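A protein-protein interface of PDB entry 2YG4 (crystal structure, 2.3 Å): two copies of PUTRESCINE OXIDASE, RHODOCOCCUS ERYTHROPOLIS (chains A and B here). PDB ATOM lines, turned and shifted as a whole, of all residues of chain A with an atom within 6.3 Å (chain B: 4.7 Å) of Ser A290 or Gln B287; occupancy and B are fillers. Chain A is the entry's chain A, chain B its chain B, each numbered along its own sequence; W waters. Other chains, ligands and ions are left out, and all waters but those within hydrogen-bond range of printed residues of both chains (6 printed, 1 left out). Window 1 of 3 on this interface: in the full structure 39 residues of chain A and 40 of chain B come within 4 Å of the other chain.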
ATOM      1  N   LEU A 174     -13.150 -13.481  -5.663  1.00  0.00           N
ATOM      2  CA  LEU A 174     -13.254 -14.799  -6.232  1.00  0.00           C
ATOM      3  C   LEU A 174     -11.887 -15.370  -6.445  1.00  0.00           C
ATOM      4  O   LEU A 174     -11.716 -16.585  -6.585  1.00  0.00           O
ATOM      5  CB  LEU A 174     -14.056 -14.720  -7.511  1.00  0.00           C
ATOM      6  CG  LEU A 174     -15.564 -14.393  -7.322  1.00  0.00           C
ATOM      7  CD1 LEU A 174     -16.345 -14.241  -8.650  1.00  0.00           C
ATOM      8  CD2 LEU A 174     -16.171 -15.506  -6.542  1.00  0.00           C
ATOM      9  N   LYS A 176      -9.844 -15.279  -8.975  1.00  0.00           N
ATOM     10  CA  LYS A 176      -9.776 -15.903 -10.257  1.00  0.00           C
ATOM     11  C   LYS A 176      -9.707 -14.780 -11.295  1.00  0.00           C
ATOM     12  O   LYS A 176     -10.224 -13.682 -11.100  1.00  0.00           O
ATOM     13  CB  LYS A 176     -11.013 -16.707 -10.506  1.00  0.00           C
ATOM     14  CG  LYS A 176     -10.994 -18.074  -9.844  1.00  0.00           C
ATOM     15  CD  LYS A 176     -12.298 -18.862 -10.117  1.00  0.00           C
ATOM     16  CE  LYS A 176     -12.237 -20.199  -9.326  1.00  0.00           C
ATOM     17  NZ  LYS A 176     -13.510 -21.021  -9.515  1.00  0.00           N
ATOM     18  N   PRO A 266     -16.268 -27.708  -1.600  1.00  0.00           N
ATOM     19  CA  PRO A 266     -16.813 -28.698  -2.547  1.00  0.00           C
ATOM     20  C   PRO A 266     -15.786 -29.344  -3.419  1.00  0.00           C
ATOM     21  O   PRO A 266     -16.041 -30.432  -3.937  1.00  0.00           O
ATOM     22  CB  PRO A 266     -17.830 -27.905  -3.372  1.00  0.00           C
ATOM     23  CG  PRO A 266     -17.452 -26.497  -3.153  1.00  0.00           C
ATOM     24  CD  PRO A 266     -16.819 -26.356  -1.800  1.00  0.00           C
ATOM     25  N   ASN A 267     -14.594 -28.751  -3.512  1.00  0.00           N
ATOM     26  CA  ASN A 267     -13.520 -29.386  -4.285  1.00  0.00           C
ATOM     27  C   ASN A 267     -12.981 -30.570  -3.552  1.00  0.00           C
ATOM     28  O   ASN A 267     -12.220 -31.331  -4.158  1.00  0.00           O
ATOM     29  CB  ASN A 267     -12.352 -28.451  -4.551  1.00  0.00           C
ATOM     30  CG  ASN A 267     -11.821 -27.878  -3.281  1.00  0.00           C
ATOM     31  OD1 ASN A 267     -12.598 -27.299  -2.519  1.00  0.00           O
ATOM     32  ND2 ASN A 267     -10.529 -28.084  -2.991  1.00  0.00           N
ATOM     33  N   HIS A 286     -19.722 -31.454  -8.977  1.00  0.00           N
ATOM     34  CA  HIS A 286     -18.581 -31.303  -8.097  1.00  0.00           C
ATOM     35  C   HIS A 286     -17.313 -31.086  -8.877  1.00  0.00           C
ATOM     36  O   HIS A 286     -16.399 -30.427  -8.368  1.00  0.00           O
ATOM     37  CB  HIS A 286     -18.425 -32.500  -7.165  1.00  0.00           C
ATOM     38  CG  HIS A 286     -19.562 -32.646  -6.196  1.00  0.00           C
ATOM     39  ND1 HIS A 286     -19.755 -33.783  -5.434  1.00  0.00           N
ATOM     40  CD2 HIS A 286     -20.572 -31.797  -5.874  1.00  0.00           C
ATOM     41  CE1 HIS A 286     -20.836 -33.628  -4.689  1.00  0.00           C
ATOM     42  NE2 HIS A 286     -21.343 -32.426  -4.927  1.00  0.00           N
ATOM     43  N   GLN A 287     -17.256 -31.581 -10.120  1.00  0.00           N
ATOM     44  CA  GLN A 287     -16.091 -31.346 -11.008  1.00  0.00           C
ATOM     45  C   GLN A 287     -16.019 -29.913 -11.468  1.00  0.00           C
ATOM     46  O   GLN A 287     -14.966 -29.471 -11.926  1.00  0.00           O
ATOM     47  CB  GLN A 287     -16.151 -32.257 -12.267  1.00  0.00           C
ATOM     48  CG  GLN A 287     -16.029 -33.712 -11.975  1.00  0.00           C
ATOM     49  CD  GLN A 287     -16.143 -34.548 -13.222  1.00  0.00           C
ATOM     50  OE1 GLN A 287     -15.314 -34.434 -14.147  1.00  0.00           O
ATOM     51  NE2 GLN A 287     -17.155 -35.432 -13.255  1.00  0.00           N
ATOM     52  N   HIS A 288     -17.128 -29.176 -11.399  1.00  0.00           N
ATOM     53  CA  HIS A 288     -17.108 -27.796 -11.882  1.00  0.00           C
ATOM     54  C   HIS A 288     -16.881 -26.722 -10.822  1.00  0.00           C
ATOM     55  O   HIS A 288     -17.093 -25.528 -11.086  1.00  0.00           O
ATOM     56  CB  HIS A 288     -18.387 -27.534 -12.655  1.00  0.00           C
ATOM     57  CG  HIS A 288     -18.479 -28.314 -13.945  1.00  0.00           C
ATOM     58  ND1 HIS A 288     -17.955 -27.863 -15.128  1.00  0.00           N
ATOM     59  CD2 HIS A 288     -19.002 -29.522 -14.219  1.00  0.00           C
ATOM     60  CE1 HIS A 288     -18.213 -28.726 -16.093  1.00  0.00           C
ATOM     61  NE2 HIS A 288     -18.857 -29.745 -15.562  1.00  0.00           N
ATOM     62  N   GLN A 289     -16.475 -27.138  -9.624  1.00  0.00           N
ATOM     63  CA  GLN A 289     -16.251 -26.223  -8.507  1.00  0.00           C
ATOM     64  C   GLN A 289     -14.743 -26.148  -8.289  1.00  0.00           C
ATOM     65  O   GLN A 289     -14.113 -27.179  -8.209  1.00  0.00           O
ATOM     66  CB  GLN A 289     -16.882 -26.762  -7.183  1.00  0.00           C
ATOM     67  CG  GLN A 289     -18.473 -26.849  -7.065  1.00  0.00           C
ATOM     68  CD  GLN A 289     -19.088 -25.558  -6.519  1.00  0.00           C
ATOM     69  OE1 GLN A 289     -18.490 -24.472  -6.645  1.00  0.00           O
ATOM     70  NE2 GLN A 289     -20.284 -25.660  -5.921  1.00  0.00           N
ATOM     71  N   SER A 290     -14.185 -24.950  -8.111  1.00  0.00           N
ATOM     72  CA  SER A 290     -12.768 -24.832  -7.769  1.00  0.00           C
ATOM     73  C   SER A 290     -12.511 -23.624  -6.925  1.00  0.00           C
ATOM     74  O   SER A 290     -13.132 -22.582  -7.100  1.00  0.00           O
ATOM     75  CB  SER A 290     -11.886 -24.727  -9.028  1.00  0.00           C
ATOM     76  OG  SER A 290     -12.442 -23.742  -9.902  1.00  0.00           O
ATOM     77  N   LEU A 291     -11.521 -23.754  -6.063  1.00  0.00           N
ATOM     78  CA  LEU A 291     -11.004 -22.622  -5.264  1.00  0.00           C
ATOM     79  C   LEU A 291     -10.183 -21.681  -6.134  1.00  0.00           C
ATOM     80  O   LEU A 291      -9.561 -22.108  -7.133  1.00  0.00           O
ATOM     81  CB  LEU A 291     -10.072 -23.148  -4.169  1.00  0.00           C
ATOM     82  CG  LEU A 291     -10.850 -24.031  -3.162  1.00  0.00           C
ATOM     83  CD1 LEU A 291      -9.847 -24.789  -2.340  1.00  0.00           C
ATOM     84  CD2 LEU A 291     -11.677 -23.142  -2.299  1.00  0.00           C
ATOM     85  N   GLY A 292     -10.206 -20.397  -5.787  1.00  0.00           N
ATOM     86  CA  GLY A 292      -9.338 -19.421  -6.449  1.00  0.00           C
ATOM     87  C   GLY A 292      -7.947 -19.581  -5.823  1.00  0.00           C
ATOM     88  O   GLY A 292      -7.673 -20.597  -5.191  1.00  0.00           O
ATOM     89  N   THR A 391      -7.373 -27.824   2.264  1.00  0.00           N
ATOM     90  CA  THR A 391      -8.030 -26.671   1.675  1.00  0.00           C
ATOM     91  C   THR A 391      -7.788 -26.616   0.159  1.00  0.00           C
ATOM     92  O   THR A 391      -8.691 -26.838  -0.602  1.00  0.00           O
ATOM     93  CB  THR A 391      -7.582 -25.386   2.350  1.00  0.00           C
ATOM     94  OG1 THR A 391      -7.671 -25.578   3.764  1.00  0.00           O
ATOM     95  CG2 THR A 391      -8.419 -24.219   1.886  1.00  0.00           C
ATOM     96  N   ARG A 392      -6.544 -26.349  -0.244  1.00  0.00           N
ATOM     97  CA  ARG A 392      -6.008 -26.346  -1.659  1.00  0.00           C
ATOM     98  C   ARG A 392      -6.291 -25.031  -2.450  1.00  0.00           C
ATOM     99  O   ARG A 392      -6.340 -25.048  -3.685  1.00  0.00           O
ATOM    100  CB  ARG A 392      -6.492 -27.558  -2.432  1.00  0.00           C
ATOM    101  CG  ARG A 392      -6.361 -28.866  -1.712  1.00  0.00           C
ATOM    102  CD  ARG A 392      -6.794 -30.101  -2.658  1.00  0.00           C
ATOM    103  NE  ARG A 392      -6.561 -31.348  -1.906  1.00  0.00           N
ATOM    104  CZ  ARG A 392      -6.276 -32.542  -2.442  1.00  0.00           C
ATOM    105  NH1 ARG A 392      -6.188 -32.699  -3.797  1.00  0.00           N
ATOM    106  NH2 ARG A 392      -6.054 -33.588  -1.600  1.00  0.00           N
ATOM    107  N   GLY A 393      -6.523 -23.912  -1.756  1.00  0.00           N
ATOM    108  CA  GLY A 393      -6.684 -22.649  -2.437  1.00  0.00           C
ATOM    109  C   GLY A 393      -7.265 -21.639  -1.524  1.00  0.00           C
ATOM    110  O   GLY A 393      -7.445 -21.937  -0.356  1.00  0.00           O
ATOM    111  N   ALA A 396     -11.989 -19.176  -1.574  1.00  0.00           N
ATOM    112  CA  ALA A 396     -13.125 -20.067  -1.512  1.00  0.00           C
ATOM    113  C   ALA A 396     -13.503 -20.587  -2.918  1.00  0.00           C
ATOM    114  O   ALA A 396     -12.922 -20.135  -3.948  1.00  0.00           O
ATOM    115  CB  ALA A 396     -14.242 -19.349  -0.908  1.00  0.00           C
ATOM    116  N   ALA A 397     -14.451 -21.510  -2.990  1.00  0.00           N
ATOM    117  CA  ALA A 397     -14.762 -22.104  -4.266  1.00  0.00           C
ATOM    118  C   ALA A 397     -15.874 -21.362  -5.013  1.00  0.00           C
ATOM    119  O   ALA A 397     -16.785 -20.769  -4.387  1.00  0.00           O
ATOM    120  CB  ALA A 397     -15.143 -23.537  -4.065  1.00  0.00           C
ATOM    121  N   SER A 398     -15.830 -21.432  -6.344  1.00  0.00           N
ATOM    122  CA  SER A 398     -16.891 -20.879  -7.220  1.00  0.00           C
ATOM    123  C   SER A 398     -16.921 -21.797  -8.448  1.00  0.00           C
ATOM    124  O   SER A 398     -15.965 -22.536  -8.702  1.00  0.00           O
ATOM    125  CB  SER A 398     -16.527 -19.437  -7.643  1.00  0.00           C
ATOM    126  OG  SER A 398     -15.221 -19.360  -8.299  1.00  0.00           O
ATOM    127  N   PHE A 399     -18.001 -21.746  -9.199  1.00  0.00           N
ATOM    128  CA  PHE A 399     -18.160 -22.531 -10.408  1.00  0.00           C
ATOM    129  C   PHE A 399     -17.187 -22.050 -11.482  1.00  0.00           C
ATOM    130  O   PHE A 399     -16.726 -20.920 -11.391  1.00  0.00           O
ATOM    131  CB  PHE A 399     -19.641 -22.389 -10.865  1.00  0.00           C
ATOM    132  CG  PHE A 399     -20.598 -23.311 -10.074  1.00  0.00           C
ATOM    133  CD1 PHE A 399     -20.497 -24.677 -10.219  1.00  0.00           C
ATOM    134  CD2 PHE A 399     -21.474 -22.804  -9.116  1.00  0.00           C
ATOM    135  CE1 PHE A 399     -21.326 -25.564  -9.484  1.00  0.00           C
ATOM    136  CE2 PHE A 399     -22.325 -23.676  -8.353  1.00  0.00           C
ATOM    137  CZ  PHE A 399     -22.232 -25.071  -8.565  1.00  0.00           C
ATOM    138  N   ASP A 400     -16.837 -22.885 -12.451  1.00  0.00           N
ATOM    139  CA  ASP A 400     -16.222 -22.388 -13.675  1.00  0.00           C
ATOM    140  C   ASP A 400     -17.333 -21.701 -14.527  1.00  0.00           C
ATOM    141  O   ASP A 400     -18.483 -21.661 -14.147  1.00  0.00           O
ATOM    142  CB  ASP A 400     -15.585 -23.525 -14.476  1.00  0.00           C
ATOM    143  CG  ASP A 400     -16.626 -24.584 -14.905  1.00  0.00           C
ATOM    144  OD1 ASP A 400     -17.782 -24.423 -14.454  1.00  0.00           O
ATOM    145  OD2 ASP A 400     -16.309 -25.556 -15.670  1.00  0.00           O
ATOM    146  N   HIS B 283      -2.459 -29.425  -6.900  1.00  0.00           N
ATOM    147  CA  HIS B 283      -3.685 -29.226  -6.105  1.00  0.00           C
ATOM    148  C   HIS B 283      -4.655 -28.272  -6.872  1.00  0.00           C
ATOM    149  O   HIS B 283      -5.892 -28.507  -6.927  1.00  0.00           O
ATOM    150  CB  HIS B 283      -3.296 -28.530  -4.805  1.00  0.00           C
ATOM    151  CG  HIS B 283      -2.929 -29.470  -3.662  1.00  0.00           C
ATOM    152  ND1 HIS B 283      -3.129 -30.842  -3.711  1.00  0.00           N
ATOM    153  CD2 HIS B 283      -2.412 -29.213  -2.431  1.00  0.00           C
ATOM    154  CE1 HIS B 283      -2.714 -31.390  -2.581  1.00  0.00           C
ATOM    155  NE2 HIS B 283      -2.265 -30.429  -1.794  1.00  0.00           N
ATOM    156  N   GLN B 284      -4.082 -27.178  -7.441  1.00  0.00           N
ATOM    157  CA  GLN B 284      -4.839 -26.129  -8.087  1.00  0.00           C
ATOM    158  C   GLN B 284      -5.253 -26.631  -9.482  1.00  0.00           C
ATOM    159  O   GLN B 284      -6.460 -26.644  -9.809  1.00  0.00           O
ATOM    160  CB  GLN B 284      -3.954 -24.883  -8.162  1.00  0.00           C
ATOM    161  CG  GLN B 284      -3.949 -24.115  -6.845  1.00  0.00           C
ATOM    162  CD  GLN B 284      -5.145 -23.107  -6.774  1.00  0.00           C
ATOM    163  OE1 GLN B 284      -6.028 -23.169  -5.859  1.00  0.00           O
ATOM    164  NE2 GLN B 284      -5.167 -22.182  -7.698  1.00  0.00           N
ATOM    165  N   MET B 285      -4.285 -27.116 -10.272  1.00  0.00           N
ATOM    166  CA  MET B 285      -4.551 -27.518 -11.651  1.00  0.00           C
ATOM    167  C   MET B 285      -5.633 -28.570 -11.752  1.00  0.00           C
ATOM    168  O   MET B 285      -6.553 -28.491 -12.606  1.00  0.00           O
ATOM    169  CB  MET B 285      -3.245 -27.992 -12.350  1.00  0.00           C
ATOM    170  CG  MET B 285      -3.490 -28.882 -13.562  1.00  0.00           C
ATOM    171  SD  MET B 285      -1.917 -29.247 -14.467  1.00  0.00           S
ATOM    172  CE  MET B 285      -1.052 -30.140 -13.198  1.00  0.00           C
ATOM    173  N   HIS B 286      -5.565 -29.558 -10.870  1.00  0.00           N
ATOM    174  CA  HIS B 286      -6.502 -30.692 -10.959  1.00  0.00           C
ATOM    175  C   HIS B 286      -7.931 -30.271 -10.682  1.00  0.00           C
ATOM    176  O   HIS B 286      -8.852 -30.911 -11.152  1.00  0.00           O
ATOM    177  CB  HIS B 286      -6.095 -31.811  -9.999  1.00  0.00           C
ATOM    178  CG  HIS B 286      -4.768 -32.420 -10.335  1.00  0.00           C
ATOM    179  ND1 HIS B 286      -4.035 -33.140  -9.424  1.00  0.00           N
ATOM    180  CD2 HIS B 286      -4.013 -32.363 -11.467  1.00  0.00           C
ATOM    181  CE1 HIS B 286      -2.919 -33.559  -9.991  1.00  0.00           C
ATOM    182  NE2 HIS B 286      -2.872 -33.085 -11.221  1.00  0.00           N
ATOM    183  N   GLN B 287      -8.121 -29.227  -9.904  1.00  0.00           N
ATOM    184  CA  GLN B 287      -9.460 -28.660  -9.691  1.00  0.00           C
ATOM    185  C   GLN B 287     -10.068 -28.039 -10.955  1.00  0.00           C
ATOM    186  O   GLN B 287     -11.295 -27.853 -11.016  1.00  0.00           O
ATOM    187  CB  GLN B 287      -9.411 -27.552  -8.605  1.00  0.00           C
ATOM    188  CG  GLN B 287      -9.142 -28.085  -7.283  1.00  0.00           C
ATOM    189  CD  GLN B 287      -9.027 -26.995  -6.238  1.00  0.00           C
ATOM    190  OE1 GLN B 287     -10.019 -26.262  -5.952  1.00  0.00           O
ATOM    191  NE2 GLN B 287      -7.815 -26.890  -5.608  1.00  0.00           N
ATOM    192  N   HIS B 288      -9.221 -27.610 -11.911  1.00  0.00           N
ATOM    193  CA  HIS B 288      -9.723 -26.905 -13.057  1.00  0.00           C
ATOM    194  C   HIS B 288      -9.953 -27.854 -14.256  1.00  0.00           C
ATOM    195  O   HIS B 288     -10.166 -27.375 -15.347  1.00  0.00           O
ATOM    196  CB  HIS B 288      -8.759 -25.837 -13.425  1.00  0.00           C
ATOM    197  CG  HIS B 288      -8.782 -24.670 -12.483  1.00  0.00           C
ATOM    198  ND1 HIS B 288      -9.764 -23.708 -12.523  1.00  0.00           N
ATOM    199  CD2 HIS B 288      -7.946 -24.306 -11.478  1.00  0.00           C
ATOM    200  CE1 HIS B 288      -9.549 -22.808 -11.576  1.00  0.00           C
ATOM    201  NE2 HIS B 288      -8.469 -23.166 -10.907  1.00  0.00           N
ATOM    202  N   GLN B 289      -9.947 -29.175 -14.040  1.00  0.00           N
ATOM    203  CA  GLN B 289     -10.119 -30.159 -15.107  1.00  0.00           C
ATOM    204  C   GLN B 289     -11.515 -30.838 -14.863  1.00  0.00           C
ATOM    205  O   GLN B 289     -11.845 -31.143 -13.738  1.00  0.00           O
ATOM    206  CB  GLN B 289      -9.010 -31.246 -15.011  1.00  0.00           C
ATOM    207  CG  GLN B 289      -7.534 -30.843 -15.447  1.00  0.00           C
ATOM    208  CD  GLN B 289      -7.229 -31.253 -16.862  1.00  0.00           C
ATOM    209  OE1 GLN B 289      -8.065 -31.096 -17.763  1.00  0.00           O
ATOM    210  NE2 GLN B 289      -6.070 -31.822 -17.086  1.00  0.00           N
ATOM    211  N   ASP B 400     -11.311 -25.794 -17.624  1.00  0.00           N
ATOM    212  CA  ASP B 400     -12.357 -24.767 -17.652  1.00  0.00           C
ATOM    213  C   ASP B 400     -11.750 -23.599 -18.448  1.00  0.00           C
ATOM    214  O   ASP B 400     -10.574 -23.701 -18.823  1.00  0.00           O
ATOM    215  CB  ASP B 400     -12.762 -24.320 -16.240  1.00  0.00           C
ATOM    216  CG  ASP B 400     -11.538 -23.874 -15.364  1.00  0.00           C
ATOM    217  OD1 ASP B 400     -10.385 -23.732 -15.889  1.00  0.00           O
ATOM    218  OD2 ASP B 400     -11.726 -23.681 -14.110  1.00  0.00           O
HETATM  219  O   HOH W   1     -13.500 -24.637 -12.019  1.00  0.00           O
HETATM  220  O   HOH W   2      -7.533 -21.297  -8.673  1.00  0.00           O
HETATM  221  O   HOH W   3     -13.503 -27.282 -12.592  1.00  0.00           O
HETATM  222  O   HOH W   4     -12.820 -21.481 -12.728  1.00  0.00           O
HETATM  223  O   HOH W   5      -4.613 -33.117  -6.726  1.00  0.00           O
HETATM  224  O   HOH W   6      -6.783 -30.917  -6.180  1.00  0.00           O
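Water W1 lies within hydrogen-bond range of the side-chain hydroxyl (OG) of Ser A290 and the side-chain carboxylate (OD2) of Asp B400. Water W2 lies within hydrogen-bond range of O of Leu A291, NE2 of Gln B284 and NE2 of His B288. Water W6 lies within hydrogen-bond range of the backbone carbonyl oxygen (O) of His B283 (2.7 Å) and the guanidinium group (NH1) of Arg A392 (3.0 Å). Water W3 lies within hydrogen-bond range of the backbone carbonyl oxygen of Gln A287 (2.7 Å) and the backbone carbonyl oxygen of Gln B287 (2.8 Å). Water W5 bridges ND1 of His B286 (2.8 Å) and NH1 of Arg A392 (3.4 Å). Water W4 bridges OD2 of Asp B400 (2.8 Å) and NZ of Lys A176 (3.3 Å).
Gln A287 touches Gln B289, but with the chains exchanged Gln A289 does not touch Gln B287 (4.03 Å). Asp B400 touches its own counterpart, Asp A400. Of the 12 pairs that touch across the chains among the printed residues, 1 has its exchanged pair printed and touching as well.
Of the 19 printed residues of chain A, 8 touch a printed residue of chain B. Printed residues of chain A that touch a printed residue of chain B: Asn A267, Gln A287, Ser A290, Leu A291, Gly A292, Arg A392, Gly A393 and Asp A400. Hydrophobic or aromatic side chains of chain A that line the printed part of chain B: Leu A291. Of the 8 printed residues of chain B, 6 touch a printed residue of chain A. Among the printed residues, no Asp or Glu carboxylate lies within 4 Å of a Lys or Arg side-chain nitrogen of the other chain.
Of the printed residues of chain A, Gln B287 touches Asn A267 (3.5 Å), Ser A290 (3.6 Å), Leu A291 (2.9 Å) and Arg A392 (3.0 Å). Of the printed residues of chain A, His B288 touches Ser A290 (3.5 Å). Of the printed residues of chain B, Gly A393 touches Gln B284. Pro A266 touches none of the printed residues of chain B.
Among the printed residues, pairs that only touch across the chains: Asp A400 with Asp B400, Ser A290 with His B288, Asn A267 with Gln B287, Gly A393 with Gln B284, Arg A392 with His B283, Ser A290 with Gln B287, Leu A291 with Gln B284 and Gln A287 with Gln B289.
N of Leu A291 lies within hydrogen-bond range of OE1 of Gln B287. The backbone carbonyl oxygen (O) of Gly A292 sits close to the side-chain amide oxygen (OE1) of Gln B284 (3.1 Å). O of Arg A392 sits close to OE1 of Gln B284 (2.9 Å). The backbone carbonyl oxygen (O) of Arg A392 is in hydrogen-bond range of the side-chain amide nitrogen (NE2) of Gln B287 (3.0 Å).
O of Ser A290 is in hydrogen-bond range of NZ of Lys A176 (2.9 Å). The side-chain amide nitrogen of Asn A267 is in hydrogen-bond range of the backbone carbonyl oxygen of Thr A391, at 3.3 Å. The side-chain carboxylate (OD2) of Asp A400 sits at hydrogen-bond distance from a ring nitrogen (ND1) of His A288. The backbone carbonyl oxygen (O) of Ser A290 is in hydrogen-bond range of the backbone NH (N) of Ser A398, at 3.0 Å. O of His B283 is in hydrogen-bond range of NE2 of Gln B287 (2.8 Å). The side-chain carboxylate (OD2) of Asp B400 sits at hydrogen-bond distance from a ring nitrogen (ND1) of His B288, 2.5 Å away.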
